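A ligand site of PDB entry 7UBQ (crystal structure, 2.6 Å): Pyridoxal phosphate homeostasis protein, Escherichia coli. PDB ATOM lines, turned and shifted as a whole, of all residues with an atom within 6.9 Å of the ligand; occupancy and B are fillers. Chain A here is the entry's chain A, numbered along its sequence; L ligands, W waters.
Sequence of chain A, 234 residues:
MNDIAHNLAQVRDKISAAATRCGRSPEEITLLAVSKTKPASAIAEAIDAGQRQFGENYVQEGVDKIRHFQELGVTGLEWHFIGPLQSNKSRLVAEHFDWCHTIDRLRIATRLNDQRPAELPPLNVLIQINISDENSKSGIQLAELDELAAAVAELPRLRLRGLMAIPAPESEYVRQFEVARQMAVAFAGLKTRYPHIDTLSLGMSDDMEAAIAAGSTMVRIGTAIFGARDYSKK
N of Thr 223 lies within hydrogen-bond range of O4 of the ligand (2.8 Å). N of Ser 205 sits close to O5 of the ligand, at 3.5 Å. The side-chain hydroxyl of Thr 223 lies within hydrogen-bond range of an oxygen (O4) of the ligand (2.7 Å). An oxygen (O1) of the ligand is in hydrogen-bond range of the side-chain amide nitrogen (ND2) of Asn 57, 3.0 Å away. The guanidinium group of Arg 229 is in salt-bridge range of an oxygen (O4) of the ligand, at 2.8 Å. An oxygen (O5) of the ligand is in hydrogen-bond range of the backbone NH (N) of Gly 222, 2.6 Å away. A nitrogen (N1) of the ligand sits at hydrogen-bond distance from the guanidinium group of Arg 220 (2.8 Å). O2 of the ligand lies close to NZ of Lys 36, at 3.4 Å. OG of Ser 205 lies within hydrogen-bond range of O5 of the ligand, 2.5 Å away.
OG of Ser 201 is in hydrogen-bond range of NH1 of Arg 220, 3.0 Å away. The backbone NH (N) of Arg 220 is in hydrogen-bond range of the backbone carbonyl oxygen (O) of Gly 203, 2.8 Å away. OG of Ser 205 is in hydrogen-bond range of N of Ala 224 (3.4 Å). SD of Met 204 sits close to NH2 of Arg 220 (3.7 Å). The side-chain hydroxyl (OH) of Tyr 58 lies within hydrogen-bond range of the side-chain amino group (NZ) of Lys 36, 3.4 Å away. The backbone carbonyl oxygen of Leu 32 sits at hydrogen-bond distance from the backbone NH of Ile 221, 2.9 Å away. N of Val 34 lies within hydrogen-bond range of O of Ile 221, 2.7 Å away.
The side-chain sulfur (SD) of Met 204 lies close to a nitrogen (N1) of the ligand, at 3.7 Å. Residues that only touch the ligand: Val 34, Ile 82, Ile 166 and Ile 221. Hydrophobic or aromatic side chains within 4 Å of the ligand: Val 34, Ile 82, Ile 166 and Met 204. 12 residues have an atom within 4 Å of the ligand: Val 34, Lys 36, Asn 57, Ile 82, Ile 166, Met 204, Ser 205, Arg 220, Ile 221, Gly 222, Thr 223 and Arg 229. Along chain A the residues within 4 Å of the ligand span positions 34 to 229. The nearest printed residue that does not touch the ligand is Ala 224 (4.7 Å).
Water W2 lies within hydrogen-bond range of the backbone NH (N) of Asp 206, an oxygen (O6) of the ligand and the backbone NH (N) of Ser 205.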
ATOM      1  N   LEU A  32      34.039  19.565  -2.746  1.00  0.00           N
ATOM      2  CA  LEU A  32      33.536  18.669  -1.715  1.00  0.00           C
ATOM      3  C   LEU A  32      32.861  17.510  -2.427  1.00  0.00           C
ATOM      4  O   LEU A  32      31.816  17.686  -3.062  1.00  0.00           O
ATOM      5  CB  LEU A  32      32.557  19.375  -0.771  1.00  0.00           C
ATOM      6  CG  LEU A  32      31.896  18.466   0.287  1.00  0.00           C
ATOM      7  CD1 LEU A  32      32.906  18.083   1.366  1.00  0.00           C
ATOM      8  CD2 LEU A  32      30.651  19.116   0.892  1.00  0.00           C
ATOM      9  N   VAL A  34      30.579  14.529  -2.799  1.00  0.00           N
ATOM     10  CA  VAL A  34      29.382  14.110  -2.066  1.00  0.00           C
ATOM     11  C   VAL A  34      29.226  12.609  -2.264  1.00  0.00           C
ATOM     12  O   VAL A  34      28.741  12.137  -3.305  1.00  0.00           O
ATOM     13  CB  VAL A  34      28.142  14.886  -2.496  1.00  0.00           C
ATOM     14  CG1 VAL A  34      26.917  14.337  -1.789  1.00  0.00           C
ATOM     15  CG2 VAL A  34      28.337  16.345  -2.119  1.00  0.00           C
ATOM     16  N   LYS A  36      27.389  10.426  -0.557  1.00  0.00           N
ATOM     17  CA  LYS A  36      26.205   9.778  -0.010  1.00  0.00           C
ATOM     18  C   LYS A  36      25.737   8.690  -0.972  1.00  0.00           C
ATOM     19  O   LYS A  36      25.799   8.846  -2.202  1.00  0.00           O
ATOM     20  CB  LYS A  36      25.087  10.784   0.270  1.00  0.00           C
ATOM     21  CG  LYS A  36      24.213  11.223  -0.888  1.00  0.00           C
ATOM     22  CD  LYS A  36      22.779  11.473  -0.381  1.00  0.00           C
ATOM     23  CE  LYS A  36      21.967  12.354  -1.332  1.00  0.00           C
ATOM     24  NZ  LYS A  36      20.552  12.559  -0.879  1.00  0.00           N
ATOM     25  N   ASN A  57      25.281  12.677   3.809  1.00  0.00           N
ATOM     26  CA  ASN A  57      23.988  13.216   4.182  1.00  0.00           C
ATOM     27  C   ASN A  57      23.305  12.475   5.323  1.00  0.00           C
ATOM     28  O   ASN A  57      22.359  13.015   5.907  1.00  0.00           O
ATOM     29  CB  ASN A  57      23.022  13.236   2.988  1.00  0.00           C
ATOM     30  CG  ASN A  57      23.515  14.094   1.856  1.00  0.00           C
ATOM     31  OD1 ASN A  57      24.694  14.052   1.500  1.00  0.00           O
ATOM     32  ND2 ASN A  57      22.616  14.896   1.277  1.00  0.00           N
ATOM     33  N   TYR A  58      23.719  11.252   5.615  1.00  0.00           N
ATOM     34  CA  TYR A  58      23.071  10.444   6.649  1.00  0.00           C
ATOM     35  C   TYR A  58      24.110  10.057   7.679  1.00  0.00           C
ATOM     36  O   TYR A  58      25.266   9.797   7.332  1.00  0.00           O
ATOM     37  CB  TYR A  58      22.378   9.237   6.039  1.00  0.00           C
ATOM     38  CG  TYR A  58      21.529   9.625   4.859  1.00  0.00           C
ATOM     39  CD1 TYR A  58      20.382  10.381   5.035  1.00  0.00           C
ATOM     40  CD2 TYR A  58      21.886   9.259   3.561  1.00  0.00           C
ATOM     41  CE1 TYR A  58      19.595  10.760   3.958  1.00  0.00           C
ATOM     42  CE2 TYR A  58      21.110   9.625   2.482  1.00  0.00           C
ATOM     43  CZ  TYR A  58      19.966  10.380   2.682  1.00  0.00           C
ATOM     44  OH  TYR A  58      19.186  10.762   1.617  1.00  0.00           O
ATOM     45  N   ILE A  82      26.183  17.070   5.572  1.00  0.00           N
ATOM     46  CA  ILE A  82      25.505  18.064   4.745  1.00  0.00           C
ATOM     47  C   ILE A  82      24.068  17.655   4.526  1.00  0.00           C
ATOM     48  O   ILE A  82      23.417  18.103   3.569  1.00  0.00           O
ATOM     49  CB  ILE A  82      26.213  18.224   3.386  1.00  0.00           C
ATOM     50  CG1 ILE A  82      26.122  16.928   2.600  1.00  0.00           C
ATOM     51  CG2 ILE A  82      27.672  18.647   3.587  1.00  0.00           C
ATOM     52  CD1 ILE A  82      26.601  17.065   1.185  1.00  0.00           C
ATOM     53  N   GLY A  83      23.558  16.789   5.391  1.00  0.00           N
ATOM     54  CA  GLY A  83      22.151  16.467   5.372  1.00  0.00           C
ATOM     55  C   GLY A  83      21.470  17.030   6.601  1.00  0.00           C
ATOM     56  O   GLY A  83      22.110  17.576   7.521  1.00  0.00           O
ATOM     57  N   HIS A 101      27.052  21.502   7.520  1.00  0.00           N
ATOM     58  CA  HIS A 101      26.520  22.575   6.676  1.00  0.00           C
ATOM     59  C   HIS A 101      25.083  22.943   6.977  1.00  0.00           C
ATOM     60  O   HIS A 101      24.551  23.838   6.302  1.00  0.00           O
ATOM     61  CB  HIS A 101      26.593  22.206   5.193  1.00  0.00           C
ATOM     62  CG  HIS A 101      27.982  22.045   4.664  1.00  0.00           C
ATOM     63  ND1 HIS A 101      28.295  22.276   3.336  1.00  0.00           N
ATOM     64  CD2 HIS A 101      29.127  21.638   5.260  1.00  0.00           C
ATOM     65  CE1 HIS A 101      29.580  22.042   3.153  1.00  0.00           C
ATOM     66  NE2 HIS A 101      30.110  21.647   4.304  1.00  0.00           N
ATOM     67  N   THR A 102      24.428  22.296   7.943  1.00  0.00           N
ATOM     68  CA  THR A 102      22.965  22.318   8.035  1.00  0.00           C
ATOM     69  C   THR A 102      22.448  22.845   9.379  1.00  0.00           C
ATOM     70  O   THR A 102      21.444  22.354   9.898  1.00  0.00           O
ATOM     71  CB  THR A 102      22.409  20.929   7.747  1.00  0.00           C
ATOM     72  OG1 THR A 102      23.117  20.008   8.576  1.00  0.00           O
ATOM     73  CG2 THR A 102      22.657  20.546   6.305  1.00  0.00           C
ATOM     74  N   GLN A 128      22.531  27.234   7.284  1.00  0.00           N
ATOM     75  CA  GLN A 128      21.852  26.889   6.032  1.00  0.00           C
ATOM     76  C   GLN A 128      20.697  27.850   5.790  1.00  0.00           C
ATOM     77  O   GLN A 128      19.852  28.031   6.672  1.00  0.00           O
ATOM     78  CB  GLN A 128      21.339  25.452   6.066  1.00  0.00           C
ATOM     79  CG  GLN A 128      20.707  24.956   4.753  1.00  0.00           C
ATOM     80  CD  GLN A 128      20.204  23.499   4.821  1.00  0.00           C
ATOM     81  OE1 GLN A 128      20.425  22.790   5.804  1.00  0.00           O
ATOM     82  NE2 GLN A 128      19.519  23.059   3.782  1.00  0.00           N
ATOM     83  N   MET A 164      25.396  27.977   3.945  1.00  0.00           N
ATOM     84  CA  MET A 164      25.080  26.970   2.937  1.00  0.00           C
ATOM     85  C   MET A 164      23.656  27.175   2.431  1.00  0.00           C
ATOM     86  O   MET A 164      22.796  27.681   3.154  1.00  0.00           O
ATOM     87  CB  MET A 164      25.241  25.548   3.481  1.00  0.00           C
ATOM     88  CG  MET A 164      25.142  24.446   2.432  1.00  0.00           C
ATOM     89  SD  MET A 164      23.469  23.816   2.235  1.00  0.00           S
ATOM     90  CE  MET A 164      23.408  22.652   3.580  1.00  0.00           C
ATOM     91  N   ALA A 165      23.416  26.776   1.185  1.00  0.00           N
ATOM     92  CA  ALA A 165      22.061  26.828   0.656  1.00  0.00           C
ATOM     93  C   ALA A 165      21.882  25.692  -0.335  1.00  0.00           C
ATOM     94  O   ALA A 165      22.799  25.375  -1.094  1.00  0.00           O
ATOM     95  CB  ALA A 165      21.760  28.174  -0.036  1.00  0.00           C
ATOM     96  N   ILE A 166      20.714  25.057  -0.292  1.00  0.00           N
ATOM     97  CA  ILE A 166      20.317  24.116  -1.327  1.00  0.00           C
ATOM     98  C   ILE A 166      19.206  24.801  -2.103  1.00  0.00           C
ATOM     99  O   ILE A 166      18.019  24.673  -1.744  1.00  0.00           O
ATOM    100  CB  ILE A 166      19.861  22.766  -0.772  1.00  0.00           C
ATOM    101  CG1 ILE A 166      20.949  22.112   0.067  1.00  0.00           C
ATOM    102  CG2 ILE A 166      19.491  21.821  -1.922  1.00  0.00           C
ATOM    103  CD1 ILE A 166      20.440  20.857   0.841  1.00  0.00           C
ATOM    104  N   SER A 201      29.086  27.535   1.025  1.00  0.00           N
ATOM    105  CA  SER A 201      28.867  26.207   0.450  1.00  0.00           C
ATOM    106  C   SER A 201      27.671  26.277  -0.496  1.00  0.00           C
ATOM    107  O   SER A 201      26.531  26.377  -0.046  1.00  0.00           O
ATOM    108  CB  SER A 201      28.634  25.174   1.543  1.00  0.00           C
ATOM    109  OG  SER A 201      28.095  23.992   0.999  1.00  0.00           O
ATOM    110  N   GLY A 203      26.362  25.240  -4.696  1.00  0.00           N
ATOM    111  CA  GLY A 203      26.559  24.741  -6.045  1.00  0.00           C
ATOM    112  C   GLY A 203      26.742  23.242  -6.123  1.00  0.00           C
ATOM    113  O   GLY A 203      27.532  22.670  -5.364  1.00  0.00           O
ATOM    114  N   MET A 204      26.010  22.579  -7.019  1.00  0.00           N
ATOM    115  CA  MET A 204      26.179  21.141  -7.210  1.00  0.00           C
ATOM    116  C   MET A 204      26.473  20.865  -8.679  1.00  0.00           C
ATOM    117  O   MET A 204      26.829  21.784  -9.424  1.00  0.00           O
ATOM    118  CB  MET A 204      24.939  20.392  -6.733  1.00  0.00           C
ATOM    119  CG  MET A 204      24.283  21.040  -5.546  1.00  0.00           C
ATOM    120  SD  MET A 204      23.133  19.999  -4.625  1.00  0.00           S
ATOM    121  CE  MET A 204      21.887  21.215  -4.275  1.00  0.00           C
ATOM    122  N   SER A 205      26.311  19.609  -9.108  1.00  0.00           N
ATOM    123  CA  SER A 205      26.767  19.205 -10.441  1.00  0.00           C
ATOM    124  C   SER A 205      26.233  20.126 -11.545  1.00  0.00           C
ATOM    125  O   SER A 205      26.986  20.520 -12.441  1.00  0.00           O
ATOM    126  CB  SER A 205      26.390  17.754 -10.708  1.00  0.00           C
ATOM    127  OG  SER A 205      27.147  16.851  -9.913  1.00  0.00           O
ATOM    128  N   ASP A 206      24.968  20.508 -11.482  1.00  0.00           N
ATOM    129  CA  ASP A 206      24.326  21.157 -12.613  1.00  0.00           C
ATOM    130  C   ASP A 206      24.182  22.668 -12.486  1.00  0.00           C
ATOM    131  O   ASP A 206      23.709  23.310 -13.430  1.00  0.00           O
ATOM    132  CB  ASP A 206      22.955  20.537 -12.849  1.00  0.00           C
ATOM    133  CG  ASP A 206      23.060  19.093 -13.247  1.00  0.00           C
ATOM    134  OD1 ASP A 206      23.928  18.781 -14.107  1.00  0.00           O
ATOM    135  OD2 ASP A 206      22.308  18.273 -12.684  1.00  0.00           O
ATOM    136  N   VAL A 219      31.888  23.909  -3.858  1.00  0.00           N
ATOM    137  CA  VAL A 219      30.856  23.187  -4.599  1.00  0.00           C
ATOM    138  C   VAL A 219      30.781  21.761  -4.081  1.00  0.00           C
ATOM    139  O   VAL A 219      31.775  21.138  -3.691  1.00  0.00           O
ATOM    140  CB  VAL A 219      31.131  23.214  -6.117  1.00  0.00           C
ATOM    141  CG1 VAL A 219      31.015  24.631  -6.625  1.00  0.00           C
ATOM    142  CG2 VAL A 219      32.495  22.632  -6.414  1.00  0.00           C
ATOM    143  N   ARG A 220      29.576  21.226  -4.084  1.00  0.00           N
ATOM    144  CA  ARG A 220      29.282  19.919  -3.524  1.00  0.00           C
ATOM    145  C   ARG A 220      28.915  19.021  -4.701  1.00  0.00           C
ATOM    146  O   ARG A 220      27.783  19.061  -5.190  1.00  0.00           O
ATOM    147  CB  ARG A 220      28.172  20.025  -2.492  1.00  0.00           C
ATOM    148  CG  ARG A 220      28.488  21.038  -1.385  1.00  0.00           C
ATOM    149  CD  ARG A 220      27.498  20.966  -0.234  1.00  0.00           C
ATOM    150  NE  ARG A 220      26.124  20.925  -0.729  1.00  0.00           N
ATOM    151  CZ  ARG A 220      25.428  21.990  -1.105  1.00  0.00           C
ATOM    152  NH1 ARG A 220      25.958  23.204  -1.023  1.00  0.00           N
ATOM    153  NH2 ARG A 220      24.206  21.824  -1.577  1.00  0.00           N
ATOM    154  N   ILE A 221      29.879  18.237  -5.170  1.00  0.00           N
ATOM    155  CA  ILE A 221      29.721  17.454  -6.393  1.00  0.00           C
ATOM    156  C   ILE A 221      29.547  15.990  -6.026  1.00  0.00           C
ATOM    157  O   ILE A 221      30.406  15.396  -5.367  1.00  0.00           O
ATOM    158  CB  ILE A 221      30.904  17.632  -7.341  1.00  0.00           C
ATOM    159  CG1 ILE A 221      31.104  19.124  -7.639  1.00  0.00           C
ATOM    160  CG2 ILE A 221      30.654  16.840  -8.619  1.00  0.00           C
ATOM    161  CD1 ILE A 221      29.822  19.833  -8.030  1.00  0.00           C
ATOM    162  N   GLY A 222      28.435  15.417  -6.467  1.00  0.00           N
ATOM    163  CA  GLY A 222      28.122  14.039  -6.185  1.00  0.00           C
ATOM    164  C   GLY A 222      28.099  13.229  -7.459  1.00  0.00           C
ATOM    165  O   GLY A 222      28.936  12.350  -7.664  1.00  0.00           O
ATOM    166  N   THR A 223      27.165  13.571  -8.356  1.00  0.00           N
ATOM    167  CA  THR A 223      26.942  12.747  -9.536  1.00  0.00           C
ATOM    168  C   THR A 223      28.131  12.781 -10.474  1.00  0.00           C
ATOM    169  O   THR A 223      28.595  11.738 -10.938  1.00  0.00           O
ATOM    170  CB  THR A 223      25.679  13.211 -10.263  1.00  0.00           C
ATOM    171  OG1 THR A 223      24.531  12.888  -9.473  1.00  0.00           O
ATOM    172  CG2 THR A 223      25.569  12.505 -11.589  1.00  0.00           C
ATOM    173  N   ALA A 224      28.656  13.967 -10.760  1.00  0.00           N
ATOM    174  CA  ALA A 224      29.736  14.066 -11.734  1.00  0.00           C
ATOM    175  C   ALA A 224      31.019  13.370 -11.280  1.00  0.00           C
ATOM    176  O   ALA A 224      31.950  13.245 -12.086  1.00  0.00           O
ATOM    177  CB  ALA A 224      30.016  15.532 -12.059  1.00  0.00           C
ATOM    178  N   ILE A 225      31.101  12.918 -10.025  1.00  0.00           N
ATOM    179  CA  ILE A 225      32.260  12.195  -9.509  1.00  0.00           C
ATOM    180  C   ILE A 225      31.987  10.696  -9.413  1.00  0.00           C
ATOM    181  O   ILE A 225      32.745   9.882  -9.959  1.00  0.00           O
ATOM    182  CB  ILE A 225      32.714  12.766  -8.154  1.00  0.00           C
ATOM    183  CG1 ILE A 225      33.442  14.092  -8.331  1.00  0.00           C
ATOM    184  CG2 ILE A 225      33.597  11.758  -7.454  1.00  0.00           C
ATOM    185  CD1 ILE A 225      33.670  14.804  -7.023  1.00  0.00           C
ATOM    186  N   GLY A 227      29.121   8.960 -10.224  1.00  0.00           N
ATOM    187  CA  GLY A 227      27.997   8.444 -10.973  1.00  0.00           C
ATOM    188  C   GLY A 227      26.670   8.787 -10.312  1.00  0.00           C
ATOM    189  O   GLY A 227      26.583   9.651  -9.435  1.00  0.00           O
ATOM    190  N   ARG A 229      22.919   7.988  -8.297  1.00  0.00           N
ATOM    191  CA  ARG A 229      22.475   7.314  -7.077  1.00  0.00           C
ATOM    192  C   ARG A 229      21.186   6.519  -7.318  1.00  0.00           C
ATOM    193  O   ARG A 229      20.948   5.483  -6.686  1.00  0.00           O
ATOM    194  CB  ARG A 229      22.279   8.317  -5.931  1.00  0.00           C
ATOM    195  CG  ARG A 229      23.570   8.939  -5.396  1.00  0.00           C
ATOM    196  CD  ARG A 229      23.298  10.118  -4.452  1.00  0.00           C
ATOM    197  NE  ARG A 229      22.340  11.070  -5.030  1.00  0.00           N
ATOM    198  CZ  ARG A 229      22.655  12.262  -5.530  1.00  0.00           C
ATOM    199  NH1 ARG A 229      23.913  12.686  -5.512  1.00  0.00           N
ATOM    200  NH2 ARG A 229      21.717  13.048  -6.040  1.00  0.00           N
HETATM  201  N1  LIG L   1      24.975  18.569  -1.739  1.00  0.00           N
HETATM  202  C1  LIG L   1      23.833  18.089  -1.136  1.00  0.00           C
HETATM  203  C2  LIG L   1      23.399  18.660   0.196  1.00  0.00           C
HETATM  204  C3  LIG L   1      23.126  17.079  -1.744  1.00  0.00           C
HETATM  205  O1  LIG L   1      21.916  16.547  -1.145  1.00  0.00           O
HETATM  206  C4  LIG L   1      23.558  16.571  -2.953  1.00  0.00           C
HETATM  207  C5  LIG L   1      22.704  15.436  -3.588  1.00  0.00           C
HETATM  208  O2  LIG L   1      21.593  15.172  -2.728  1.00  0.00           O
HETATM  209  C6  LIG L   1      24.699  17.073  -3.553  1.00  0.00           C
HETATM  210  C7  LIG L   1      25.406  18.076  -2.909  1.00  0.00           C
HETATM  211  C8  LIG L   1      25.243  16.551  -4.871  1.00  0.00           C
HETATM  212  O3  LIG L   1      24.371  16.663  -5.972  1.00  0.00           O
HETATM  213  P1  LIG L   1      24.873  16.096  -7.386  1.00  0.00           P
HETATM  214  O4  LIG L   1      24.772  14.623  -7.370  1.00  0.00           O
HETATM  215  O5  LIG L   1      26.308  16.486  -7.625  1.00  0.00           O
HETATM  216  O6  LIG L   1      24.003  16.659  -8.519  1.00  0.00           O
HETATM  217  O   HOH W   1      19.153  17.731  -2.278  1.00  0.00           O
HETATM  218  O   HOH W   2      23.317  19.081  -9.946  1.00  0.00           O
